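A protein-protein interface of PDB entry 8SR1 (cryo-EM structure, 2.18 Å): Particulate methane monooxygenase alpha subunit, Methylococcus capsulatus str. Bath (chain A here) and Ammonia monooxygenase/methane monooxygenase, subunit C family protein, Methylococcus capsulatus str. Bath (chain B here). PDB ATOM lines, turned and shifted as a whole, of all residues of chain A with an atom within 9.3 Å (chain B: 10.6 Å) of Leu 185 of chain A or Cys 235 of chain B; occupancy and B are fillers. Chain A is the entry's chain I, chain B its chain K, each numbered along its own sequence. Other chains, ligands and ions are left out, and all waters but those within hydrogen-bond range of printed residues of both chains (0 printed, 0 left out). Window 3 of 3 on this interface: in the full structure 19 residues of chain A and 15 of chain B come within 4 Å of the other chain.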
ATOM      1  N   ILE A 179       1.287 -20.302  -3.838  1.00  0.00           N
ATOM      2  CA  ILE A 179       2.531 -19.862  -4.461  1.00  0.00           C
ATOM      3  C   ILE A 179       2.482 -18.423  -4.962  1.00  0.00           C
ATOM      4  O   ILE A 179       3.251 -17.576  -4.498  1.00  0.00           O
ATOM      5  CB  ILE A 179       2.916 -20.807  -5.613  1.00  0.00           C
ATOM      6  CG1 ILE A 179       3.012 -22.248  -5.111  1.00  0.00           C
ATOM      7  CG2 ILE A 179       4.230 -20.372  -6.245  1.00  0.00           C
ATOM      8  CD1 ILE A 179       3.011 -23.274  -6.217  1.00  0.00           C
ATOM      9  N   PHE A 180       1.610 -18.124  -5.926  1.00  0.00           N
ATOM     10  CA  PHE A 180       1.782 -16.903  -6.707  1.00  0.00           C
ATOM     11  C   PHE A 180       0.872 -15.754  -6.284  1.00  0.00           C
ATOM     12  O   PHE A 180       1.358 -14.713  -5.837  1.00  0.00           O
ATOM     13  CB  PHE A 180       1.577 -17.215  -8.194  1.00  0.00           C
ATOM     14  CG  PHE A 180       2.746 -17.902  -8.830  1.00  0.00           C
ATOM     15  CD1 PHE A 180       3.965 -17.258  -8.942  1.00  0.00           C
ATOM     16  CD2 PHE A 180       2.629 -19.195  -9.309  1.00  0.00           C
ATOM     17  CE1 PHE A 180       5.044 -17.889  -9.525  1.00  0.00           C
ATOM     18  CE2 PHE A 180       3.707 -19.830  -9.893  1.00  0.00           C
ATOM     19  CZ  PHE A 180       4.917 -19.176 -10.000  1.00  0.00           C
ATOM     20  N   ILE A 181      -0.441 -15.924  -6.388  1.00  0.00           N
ATOM     21  CA  ILE A 181      -1.332 -14.768  -6.299  1.00  0.00           C
ATOM     22  C   ILE A 181      -1.524 -14.324  -4.851  1.00  0.00           C
ATOM     23  O   ILE A 181      -1.418 -13.119  -4.573  1.00  0.00           O
ATOM     24  CB  ILE A 181      -2.679 -15.041  -6.988  1.00  0.00           C
ATOM     25  CG1 ILE A 181      -2.484 -15.167  -8.500  1.00  0.00           C
ATOM     26  CG2 ILE A 181      -3.643 -13.908  -6.705  1.00  0.00           C
ATOM     27  CD1 ILE A 181      -3.762 -15.030  -9.300  1.00  0.00           C
ATOM     28  N   PRO A 182      -1.832 -15.218  -3.900  1.00  0.00           N
ATOM     29  CA  PRO A 182      -1.914 -14.754  -2.504  1.00  0.00           C
ATOM     30  C   PRO A 182      -0.613 -14.173  -1.983  1.00  0.00           C
ATOM     31  O   PRO A 182      -0.639 -13.179  -1.248  1.00  0.00           O
ATOM     32  CB  PRO A 182      -2.328 -16.019  -1.736  1.00  0.00           C
ATOM     33  CG  PRO A 182      -1.980 -17.144  -2.626  1.00  0.00           C
ATOM     34  CD  PRO A 182      -2.190 -16.642  -4.009  1.00  0.00           C
ATOM     35  N   ARG A 183       0.534 -14.747  -2.356  1.00  0.00           N
ATOM     36  CA  ARG A 183       1.808 -14.187  -1.912  1.00  0.00           C
ATOM     37  C   ARG A 183       2.056 -12.822  -2.539  1.00  0.00           C
ATOM     38  O   ARG A 183       2.555 -11.908  -1.875  1.00  0.00           O
ATOM     39  CB  ARG A 183       2.955 -15.146  -2.233  1.00  0.00           C
ATOM     40  CG  ARG A 183       2.989 -16.384  -1.354  1.00  0.00           C
ATOM     41  CD  ARG A 183       4.198 -17.252  -1.643  1.00  0.00           C
ATOM     42  NE  ARG A 183       5.378 -16.821  -0.905  1.00  0.00           N
ATOM     43  CZ  ARG A 183       5.737 -17.299   0.278  1.00  0.00           C
ATOM     44  NH1 ARG A 183       5.016 -18.217   0.900  1.00  0.00           N
ATOM     45  NH2 ARG A 183       6.847 -16.843   0.853  1.00  0.00           N
ATOM     46  N   LEU A 184       1.708 -12.665  -3.820  1.00  0.00           N
ATOM     47  CA  LEU A 184       1.833 -11.367  -4.472  1.00  0.00           C
ATOM     48  C   LEU A 184       0.963 -10.323  -3.782  1.00  0.00           C
ATOM     49  O   LEU A 184       1.403  -9.193  -3.543  1.00  0.00           O
ATOM     50  CB  LEU A 184       1.450 -11.489  -5.944  1.00  0.00           C
ATOM     51  CG  LEU A 184       1.299 -10.206  -6.759  1.00  0.00           C
ATOM     52  CD1 LEU A 184       2.654  -9.570  -7.004  1.00  0.00           C
ATOM     53  CD2 LEU A 184       0.589 -10.487  -8.072  1.00  0.00           C
ATOM     54  N   LEU A 185      -0.278 -10.692  -3.454  1.00  0.00           N
ATOM     55  CA  LEU A 185      -1.173  -9.763  -2.774  1.00  0.00           C
ATOM     56  C   LEU A 185      -0.659  -9.412  -1.383  1.00  0.00           C
ATOM     57  O   LEU A 185      -0.757  -8.260  -0.952  1.00  0.00           O
ATOM     58  CB  LEU A 185      -2.580 -10.352  -2.692  1.00  0.00           C
ATOM     59  CG  LEU A 185      -3.353 -10.441  -4.008  1.00  0.00           C
ATOM     60  CD1 LEU A 185      -4.652 -11.201  -3.814  1.00  0.00           C
ATOM     61  CD2 LEU A 185      -3.615  -9.059  -4.574  1.00  0.00           C
ATOM     62  N   MET A 186      -0.117 -10.396  -0.663  1.00  0.00           N
ATOM     63  CA  MET A 186       0.434 -10.123   0.660  1.00  0.00           C
ATOM     64  C   MET A 186       1.631  -9.183   0.579  1.00  0.00           C
ATOM     65  O   MET A 186       1.768  -8.275   1.407  1.00  0.00           O
ATOM     66  CB  MET A 186       0.830 -11.431   1.346  1.00  0.00           C
ATOM     67  CG  MET A 186      -0.348 -12.234   1.868  1.00  0.00           C
ATOM     68  SD  MET A 186      -0.999 -11.566   3.407  1.00  0.00           S
ATOM     69  CE  MET A 186       0.375 -11.876   4.512  1.00  0.00           C
ATOM     70  N   VAL A 187       2.506  -9.388  -0.406  1.00  0.00           N
ATOM     71  CA  VAL A 187       3.671  -8.515  -0.548  1.00  0.00           C
ATOM     72  C   VAL A 187       3.243  -7.107  -0.938  1.00  0.00           C
ATOM     73  O   VAL A 187       3.769  -6.118  -0.414  1.00  0.00           O
ATOM     74  CB  VAL A 187       4.664  -9.110  -1.562  1.00  0.00           C
ATOM     75  CG1 VAL A 187       5.758  -8.108  -1.882  1.00  0.00           C
ATOM     76  CG2 VAL A 187       5.270 -10.396  -1.020  1.00  0.00           C
ATOM     77  N   ASP A 188       2.278  -6.986  -1.854  1.00  0.00           N
ATOM     78  CA  ASP A 188       1.847  -5.665  -2.318  1.00  0.00           C
ATOM     79  C   ASP A 188       1.099  -4.908  -1.225  1.00  0.00           C
ATOM     80  O   ASP A 188       1.493  -3.805  -0.831  1.00  0.00           O
ATOM     81  CB  ASP A 188       0.977  -5.808  -3.570  1.00  0.00           C
ATOM     82  CG  ASP A 188       1.778  -6.202  -4.794  1.00  0.00           C
ATOM     83  OD1 ASP A 188       2.927  -5.734  -4.933  1.00  0.00           O
ATOM     84  OD2 ASP A 188       1.256  -6.977  -5.621  1.00  0.00           O
ATOM     85  N   ALA A 189       0.010  -5.489  -0.724  1.00  0.00           N
ATOM     86  CA  ALA A 189      -0.818  -4.820   0.274  1.00  0.00           C
ATOM     87  C   ALA A 189      -0.149  -4.855   1.639  1.00  0.00           C
ATOM     88  O   ALA A 189      -0.308  -5.818   2.395  1.00  0.00           O
ATOM     89  CB  ALA A 189      -2.204  -5.465   0.341  1.00  0.00           C
ATOM     90  N   GLY A 190       0.603  -3.806   1.959  1.00  0.00           N
ATOM     91  CA  GLY A 190       1.303  -3.730   3.223  1.00  0.00           C
ATOM     92  C   GLY A 190       2.585  -4.539   3.220  1.00  0.00           C
ATOM     93  O   GLY A 190       2.939  -5.218   2.257  1.00  0.00           O
ATOM     94  N   ARG A 191       3.296  -4.451   4.340  1.00  0.00           N
ATOM     95  CA  ARG A 191       4.505  -5.238   4.518  1.00  0.00           C
ATOM     96  C   ARG A 191       4.144  -6.716   4.611  1.00  0.00           C
ATOM     97  O   ARG A 191       3.138  -7.097   5.215  1.00  0.00           O
ATOM     98  CB  ARG A 191       5.245  -4.791   5.777  1.00  0.00           C
ATOM     99  CG  ARG A 191       6.012  -3.493   5.621  1.00  0.00           C
ATOM    100  CD  ARG A 191       6.579  -3.039   6.954  1.00  0.00           C
ATOM    101  NE  ARG A 191       7.365  -1.819   6.827  1.00  0.00           N
ATOM    102  CZ  ARG A 191       7.391  -0.852   7.735  1.00  0.00           C
ATOM    103  NH1 ARG A 191       6.690  -0.936   8.853  1.00  0.00           N
ATOM    104  NH2 ARG A 191       8.133   0.229   7.510  1.00  0.00           N
ATOM    105  N   ALA A 192       4.975  -7.563   4.003  1.00  0.00           N
ATOM    106  CA  ALA A 192       4.624  -8.974   4.002  1.00  0.00           C
ATOM    107  C   ALA A 192       5.036  -9.637   5.306  1.00  0.00           C
ATOM    108  O   ALA A 192       4.180  -9.947   6.139  1.00  0.00           O
ATOM    109  CB  ALA A 192       5.286  -9.682   2.820  1.00  0.00           C
ATOM    110  N   GLU A 194       5.448 -12.136   6.700  1.00  0.00           N
ATOM    111  CA  GLU A 194       4.603 -13.167   7.289  1.00  0.00           C
ATOM    112  C   GLU A 194       4.720 -14.479   6.530  1.00  0.00           C
ATOM    113  O   GLU A 194       4.454 -15.550   7.081  1.00  0.00           O
ATOM    114  CB  GLU A 194       3.147 -12.704   7.327  1.00  0.00           C
ATOM    115  CG  GLU A 194       2.809 -11.841   8.533  1.00  0.00           C
ATOM    116  CD  GLU A 194       1.826 -10.735   8.205  1.00  0.00           C
ATOM    117  OE1 GLU A 194       0.714 -11.049   7.733  1.00  0.00           O
ATOM    118  OE2 GLU A 194       2.167  -9.552   8.418  1.00  0.00           O
ATOM    119  N   LEU A 195       5.113 -14.405   5.259  1.00  0.00           N
ATOM    120  CA  LEU A 195       5.238 -15.599   4.441  1.00  0.00           C
ATOM    121  C   LEU A 195       6.611 -16.247   4.551  1.00  0.00           C
ATOM    122  O   LEU A 195       6.794 -17.366   4.062  1.00  0.00           O
ATOM    123  CB  LEU A 195       4.929 -15.269   2.979  1.00  0.00           C
ATOM    124  CG  LEU A 195       3.688 -14.389   2.799  1.00  0.00           C
ATOM    125  CD1 LEU A 195       4.090 -12.975   2.429  1.00  0.00           C
ATOM    126  CD2 LEU A 195       2.721 -14.963   1.787  1.00  0.00           C
ATOM    127  N   THR B 219       3.002 -11.276 -13.867  1.00  0.00           N
ATOM    128  CA  THR B 219       2.400 -10.448 -12.823  1.00  0.00           C
ATOM    129  C   THR B 219       1.248  -9.621 -13.381  1.00  0.00           C
ATOM    130  O   THR B 219       0.251  -9.390 -12.678  1.00  0.00           O
ATOM    131  CB  THR B 219       3.446  -9.560 -12.142  1.00  0.00           C
ATOM    132  OG1 THR B 219       2.791  -8.653 -11.245  1.00  0.00           O
ATOM    133  CG2 THR B 219       4.227  -8.767 -13.140  1.00  0.00           C
ATOM    134  N   THR B 221      -0.789 -10.757 -15.757  1.00  0.00           N
ATOM    135  CA  THR B 221      -1.897 -11.709 -15.804  1.00  0.00           C
ATOM    136  C   THR B 221      -2.440 -12.014 -14.417  1.00  0.00           C
ATOM    137  O   THR B 221      -3.634 -12.280 -14.270  1.00  0.00           O
ATOM    138  CB  THR B 221      -1.497 -13.020 -16.489  1.00  0.00           C
ATOM    139  OG1 THR B 221      -0.754 -13.839 -15.577  1.00  0.00           O
ATOM    140  CG2 THR B 221      -0.703 -12.779 -17.752  1.00  0.00           C
ATOM    141  N   PHE B 222      -1.586 -12.003 -13.394  1.00  0.00           N
ATOM    142  CA  PHE B 222      -2.067 -12.183 -12.029  1.00  0.00           C
ATOM    143  C   PHE B 222      -2.988 -11.039 -11.628  1.00  0.00           C
ATOM    144  O   PHE B 222      -4.049 -11.257 -11.032  1.00  0.00           O
ATOM    145  CB  PHE B 222      -0.885 -12.285 -11.065  1.00  0.00           C
ATOM    146  CG  PHE B 222      -0.122 -13.567 -11.179  1.00  0.00           C
ATOM    147  CD1 PHE B 222      -0.723 -14.703 -11.690  1.00  0.00           C
ATOM    148  CD2 PHE B 222       1.201 -13.635 -10.777  1.00  0.00           C
ATOM    149  CE1 PHE B 222      -0.019 -15.883 -11.796  1.00  0.00           C
ATOM    150  CE2 PHE B 222       1.908 -14.813 -10.882  1.00  0.00           C
ATOM    151  CZ  PHE B 222       1.299 -15.937 -11.392  1.00  0.00           C
ATOM    152  N   TYR B 223      -2.593  -9.805 -11.952  1.00  0.00           N
ATOM    153  CA  TYR B 223      -3.458  -8.664 -11.671  1.00  0.00           C
ATOM    154  C   TYR B 223      -4.761  -8.747 -12.460  1.00  0.00           C
ATOM    155  O   TYR B 223      -5.832  -8.409 -11.943  1.00  0.00           O
ATOM    156  CB  TYR B 223      -2.724  -7.358 -11.976  1.00  0.00           C
ATOM    157  CG  TYR B 223      -1.703  -6.988 -10.932  1.00  0.00           C
ATOM    158  CD1 TYR B 223      -1.930  -7.250  -9.587  1.00  0.00           C
ATOM    159  CD2 TYR B 223      -0.510  -6.376 -11.285  1.00  0.00           C
ATOM    160  CE1 TYR B 223      -1.001  -6.914  -8.625  1.00  0.00           C
ATOM    161  CE2 TYR B 223       0.430  -6.037 -10.331  1.00  0.00           C
ATOM    162  CZ  TYR B 223       0.177  -6.311  -9.003  1.00  0.00           C
ATOM    163  OH  TYR B 223       1.111  -5.970  -8.052  1.00  0.00           O
ATOM    164  N   SER B 224      -4.686  -9.194 -13.716  1.00  0.00           N
ATOM    165  CA  SER B 224      -5.894  -9.362 -14.518  1.00  0.00           C
ATOM    166  C   SER B 224      -6.811 -10.431 -13.936  1.00  0.00           C
ATOM    167  O   SER B 224      -8.037 -10.272 -13.954  1.00  0.00           O
ATOM    168  CB  SER B 224      -5.519  -9.707 -15.959  1.00  0.00           C
ATOM    169  OG  SER B 224      -6.489 -10.547 -16.554  1.00  0.00           O
ATOM    170  N   PHE B 225      -6.235 -11.522 -13.437  1.00  0.00           N
ATOM    171  CA  PHE B 225      -7.009 -12.542 -12.739  1.00  0.00           C
ATOM    172  C   PHE B 225      -7.682 -11.962 -11.505  1.00  0.00           C
ATOM    173  O   PHE B 225      -8.864 -12.223 -11.250  1.00  0.00           O
ATOM    174  CB  PHE B 225      -6.093 -13.699 -12.339  1.00  0.00           C
ATOM    175  CG  PHE B 225      -6.205 -14.908 -13.220  1.00  0.00           C
ATOM    176  CD1 PHE B 225      -7.324 -15.717 -13.166  1.00  0.00           C
ATOM    177  CD2 PHE B 225      -5.179 -15.247 -14.084  1.00  0.00           C
ATOM    178  CE1 PHE B 225      -7.423 -16.840 -13.966  1.00  0.00           C
ATOM    179  CE2 PHE B 225      -5.274 -16.365 -14.888  1.00  0.00           C
ATOM    180  CZ  PHE B 225      -6.397 -17.162 -14.829  1.00  0.00           C
ATOM    181  N   ALA B 226      -6.945 -11.174 -10.731  1.00  0.00           N
ATOM    182  CA  ALA B 226      -7.439 -10.595  -9.484  1.00  0.00           C
ATOM    183  C   ALA B 226      -8.031  -9.209  -9.702  1.00  0.00           C
ATOM    184  O   ALA B 226      -7.662  -8.250  -9.027  1.00  0.00           O
ATOM    185  CB  ALA B 226      -6.314 -10.552  -8.459  1.00  0.00           C
ATOM    186  N   GLN B 227      -8.961  -9.078 -10.646  1.00  0.00           N
ATOM    187  CA  GLN B 227      -9.602  -7.781 -10.905  1.00  0.00           C
ATOM    188  C   GLN B 227     -10.920  -7.672 -10.144  1.00  0.00           C
ATOM    189  O   GLN B 227     -11.058  -6.844  -9.239  1.00  0.00           O
ATOM    190  CB  GLN B 227      -9.820  -7.591 -12.409  1.00  0.00           C
ATOM    191  CG  GLN B 227      -8.609  -7.084 -13.189  1.00  0.00           C
ATOM    192  CD  GLN B 227      -8.216  -5.658 -12.844  1.00  0.00           C
ATOM    193  OE1 GLN B 227      -7.953  -5.327 -11.688  1.00  0.00           O
ATOM    194  NE2 GLN B 227      -8.179  -4.799 -13.858  1.00  0.00           N
ATOM    195  N   GLY B 228     -11.892  -8.507 -10.498  1.00  0.00           N
ATOM    196  CA  GLY B 228     -13.155  -8.541  -9.787  1.00  0.00           C
ATOM    197  C   GLY B 228     -13.295  -9.771  -8.921  1.00  0.00           C
ATOM    198  O   GLY B 228     -13.775  -9.699  -7.787  1.00  0.00           O
ATOM    199  N   GLY B 229     -12.863 -10.912  -9.451  1.00  0.00           N
ATOM    200  CA  GLY B 229     -12.921 -12.161  -8.725  1.00  0.00           C
ATOM    201  C   GLY B 229     -11.623 -12.482  -8.015  1.00  0.00           C
ATOM    202  O   GLY B 229     -11.214 -13.644  -7.949  1.00  0.00           O
ATOM    203  N   LEU B 230     -10.962 -11.452  -7.486  1.00  0.00           N
ATOM    204  CA  LEU B 230      -9.739 -11.661  -6.722  1.00  0.00           C
ATOM    205  C   LEU B 230      -9.980 -12.507  -5.484  1.00  0.00           C
ATOM    206  O   LEU B 230      -9.033 -13.112  -4.966  1.00  0.00           O
ATOM    207  CB  LEU B 230      -9.127 -10.311  -6.333  1.00  0.00           C
ATOM    208  CG  LEU B 230      -9.629  -9.514  -5.126  1.00  0.00           C
ATOM    209  CD1 LEU B 230      -8.866  -9.878  -3.856  1.00  0.00           C
ATOM    210  CD2 LEU B 230      -9.540  -8.017  -5.399  1.00  0.00           C
ATOM    211  N   GLY B 231     -11.217 -12.563  -5.003  1.00  0.00           N
ATOM    212  CA  GLY B 231     -11.568 -13.386  -3.868  1.00  0.00           C
ATOM    213  C   GLY B 231     -13.049 -13.295  -3.581  1.00  0.00           C
ATOM    214  O   GLY B 231     -13.880 -13.251  -4.492  1.00  0.00           O
ATOM    215  N   GLN B 232     -13.373 -13.233  -2.296  1.00  0.00           N
ATOM    216  CA  GLN B 232     -12.346 -13.124  -1.271  1.00  0.00           C
ATOM    217  C   GLN B 232     -11.991 -14.471  -0.661  1.00  0.00           C
ATOM    218  O   GLN B 232     -12.616 -15.487  -0.980  1.00  0.00           O
ATOM    219  CB  GLN B 232     -12.784 -12.149  -0.182  1.00  0.00           C
ATOM    220  CG  GLN B 232     -12.879 -10.711  -0.660  1.00  0.00           C
ATOM    221  CD  GLN B 232     -11.729 -10.327  -1.574  1.00  0.00           C
ATOM    222  OE1 GLN B 232     -11.887 -10.251  -2.790  1.00  0.00           O
ATOM    223  NE2 GLN B 232     -10.562 -10.086  -0.986  1.00  0.00           N
ATOM    224  N   SER B 233     -11.039 -14.414   0.275  1.00  0.00           N
ATOM    225  CA  SER B 233     -10.166 -15.497   0.727  1.00  0.00           C
ATOM    226  C   SER B 233      -8.748 -14.949   0.726  1.00  0.00           C
ATOM    227  O   SER B 233      -8.172 -14.670   1.782  1.00  0.00           O
ATOM    228  CB  SER B 233     -10.233 -16.742  -0.164  1.00  0.00           C
ATOM    229  OG  SER B 233      -9.084 -17.551   0.009  1.00  0.00           O
ATOM    230  N   LEU B 234      -8.186 -14.817  -0.471  1.00  0.00           N
ATOM    231  CA  LEU B 234      -6.923 -14.116  -0.666  1.00  0.00           C
ATOM    232  C   LEU B 234      -6.996 -12.729  -0.051  1.00  0.00           C
ATOM    233  O   LEU B 234      -7.884 -11.934  -0.388  1.00  0.00           O
ATOM    234  CB  LEU B 234      -6.606 -14.023  -2.164  1.00  0.00           C
ATOM    235  CG  LEU B 234      -6.285 -15.256  -3.024  1.00  0.00           C
ATOM    236  CD1 LEU B 234      -7.299 -16.390  -2.914  1.00  0.00           C
ATOM    237  CD2 LEU B 234      -6.164 -14.829  -4.470  1.00  0.00           C
ATOM    238  N   CYS B 235      -6.064 -12.442   0.858  1.00  0.00           N
ATOM    239  CA  CYS B 235      -6.048 -11.192   1.620  1.00  0.00           C
ATOM    240  C   CYS B 235      -7.355 -11.002   2.389  1.00  0.00           C
ATOM    241  O   CYS B 235      -7.864  -9.889   2.544  1.00  0.00           O
ATOM    242  CB  CYS B 235      -5.765  -9.994   0.711  1.00  0.00           C
ATOM    243  SG  CYS B 235      -4.010  -9.600   0.524  1.00  0.00           S
ATOM    244  N   GLU B 236      -7.899 -12.113   2.878  1.00  0.00           N
ATOM    245  CA  GLU B 236      -9.068 -12.094   3.752  1.00  0.00           C
ATOM    246  C   GLU B 236      -9.198 -13.416   4.500  1.00  0.00           C
ATOM    247  O   GLU B 236      -8.547 -13.630   5.522  1.00  0.00           O
ATOM    248  CB  GLU B 236     -10.351 -11.815   2.965  1.00  0.00           C
ATOM    249  CG  GLU B 236     -11.355 -10.972   3.740  1.00  0.00           C
ATOM    250  CD  GLU B 236     -12.475 -10.431   2.873  1.00  0.00           C
ATOM    251  OE1 GLU B 236     -13.476 -11.151   2.678  1.00  0.00           O
ATOM    252  OE2 GLU B 236     -12.353  -9.289   2.381  1.00  0.00           O
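Leu 185 of chain A touches just these residues of chain B: Leu 234 (3.8 Å) and Cys 235 (3.6 Å).
Cys 235 of chain B touches just one residue of chain A: Leu 185 (3.6 Å).
Ala 189 of chain A touches none of the printed residues of chain B.
No residue of chain B comes within 4 Å of Gly 190 of chain A.
Printed residues of chain A within 4 Å of Tyr 223 of chain B: Leu 184 (3.9 Å) and Asp 188 (2.6 Å).
Of the printed residues of chain A, Leu 234 of chain B touches Ile 181 and Leu 185.
Printed residues of chain B within 4 Å of Phe 180 of chain A: Phe 222 (3.5 Å).
The nearest residue of chain A that does not touch Cys 235 of chain B is Met 186 of chain A (4.1 Å).
The side-chain amide nitrogen of Gln 232 of chain B sits at hydrogen-bond distance from the backbone carbonyl oxygen of Leu 234 of chain B, 3.3 Å away.
Of the 16 printed residues of chain A, 5 touch a printed residue of chain B.
Hydrophobic or aromatic side chains of chain A within 4 Å of the printed part of chain B: Phe 180, Ile 181, Leu 184 and Leu 185.
Of the 17 printed residues of chain B, 4 touch a printed residue of chain A.
Among the printed residues, no Asp or Glu carboxylate lies within 4 Å of a Lys or Arg side-chain nitrogen of the other chain.
The side-chain carboxylate of Asp 188 of chain A sits at hydrogen-bond distance from the side-chain hydroxyl of Tyr 223 of chain B, 2.6 Å away.
Phe 222 of chain B touches Phe 180 of chain A.
CG1 of Ile 181 of chain A touches CD1 of Phe 222 of chain B (3.7 Å).
Ile 181 of chain A touches Leu 234 of chain B (CG2 to CD2, 3.5 Å).
Leu 184 of chain A touches Phe 222 of chain B (CD2 to CB, 3.8 Å).
CE1 of Tyr 223 of chain B touches CD2 of Leu 184 of chain A, at 3.9 Å.
Leu 234 of chain B touches Leu 185 of chain A (CB to CD1, 3.8 Å).
CB of Leu 185 of chain A touches SG of Cys 235 of chain B, at 3.6 Å.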
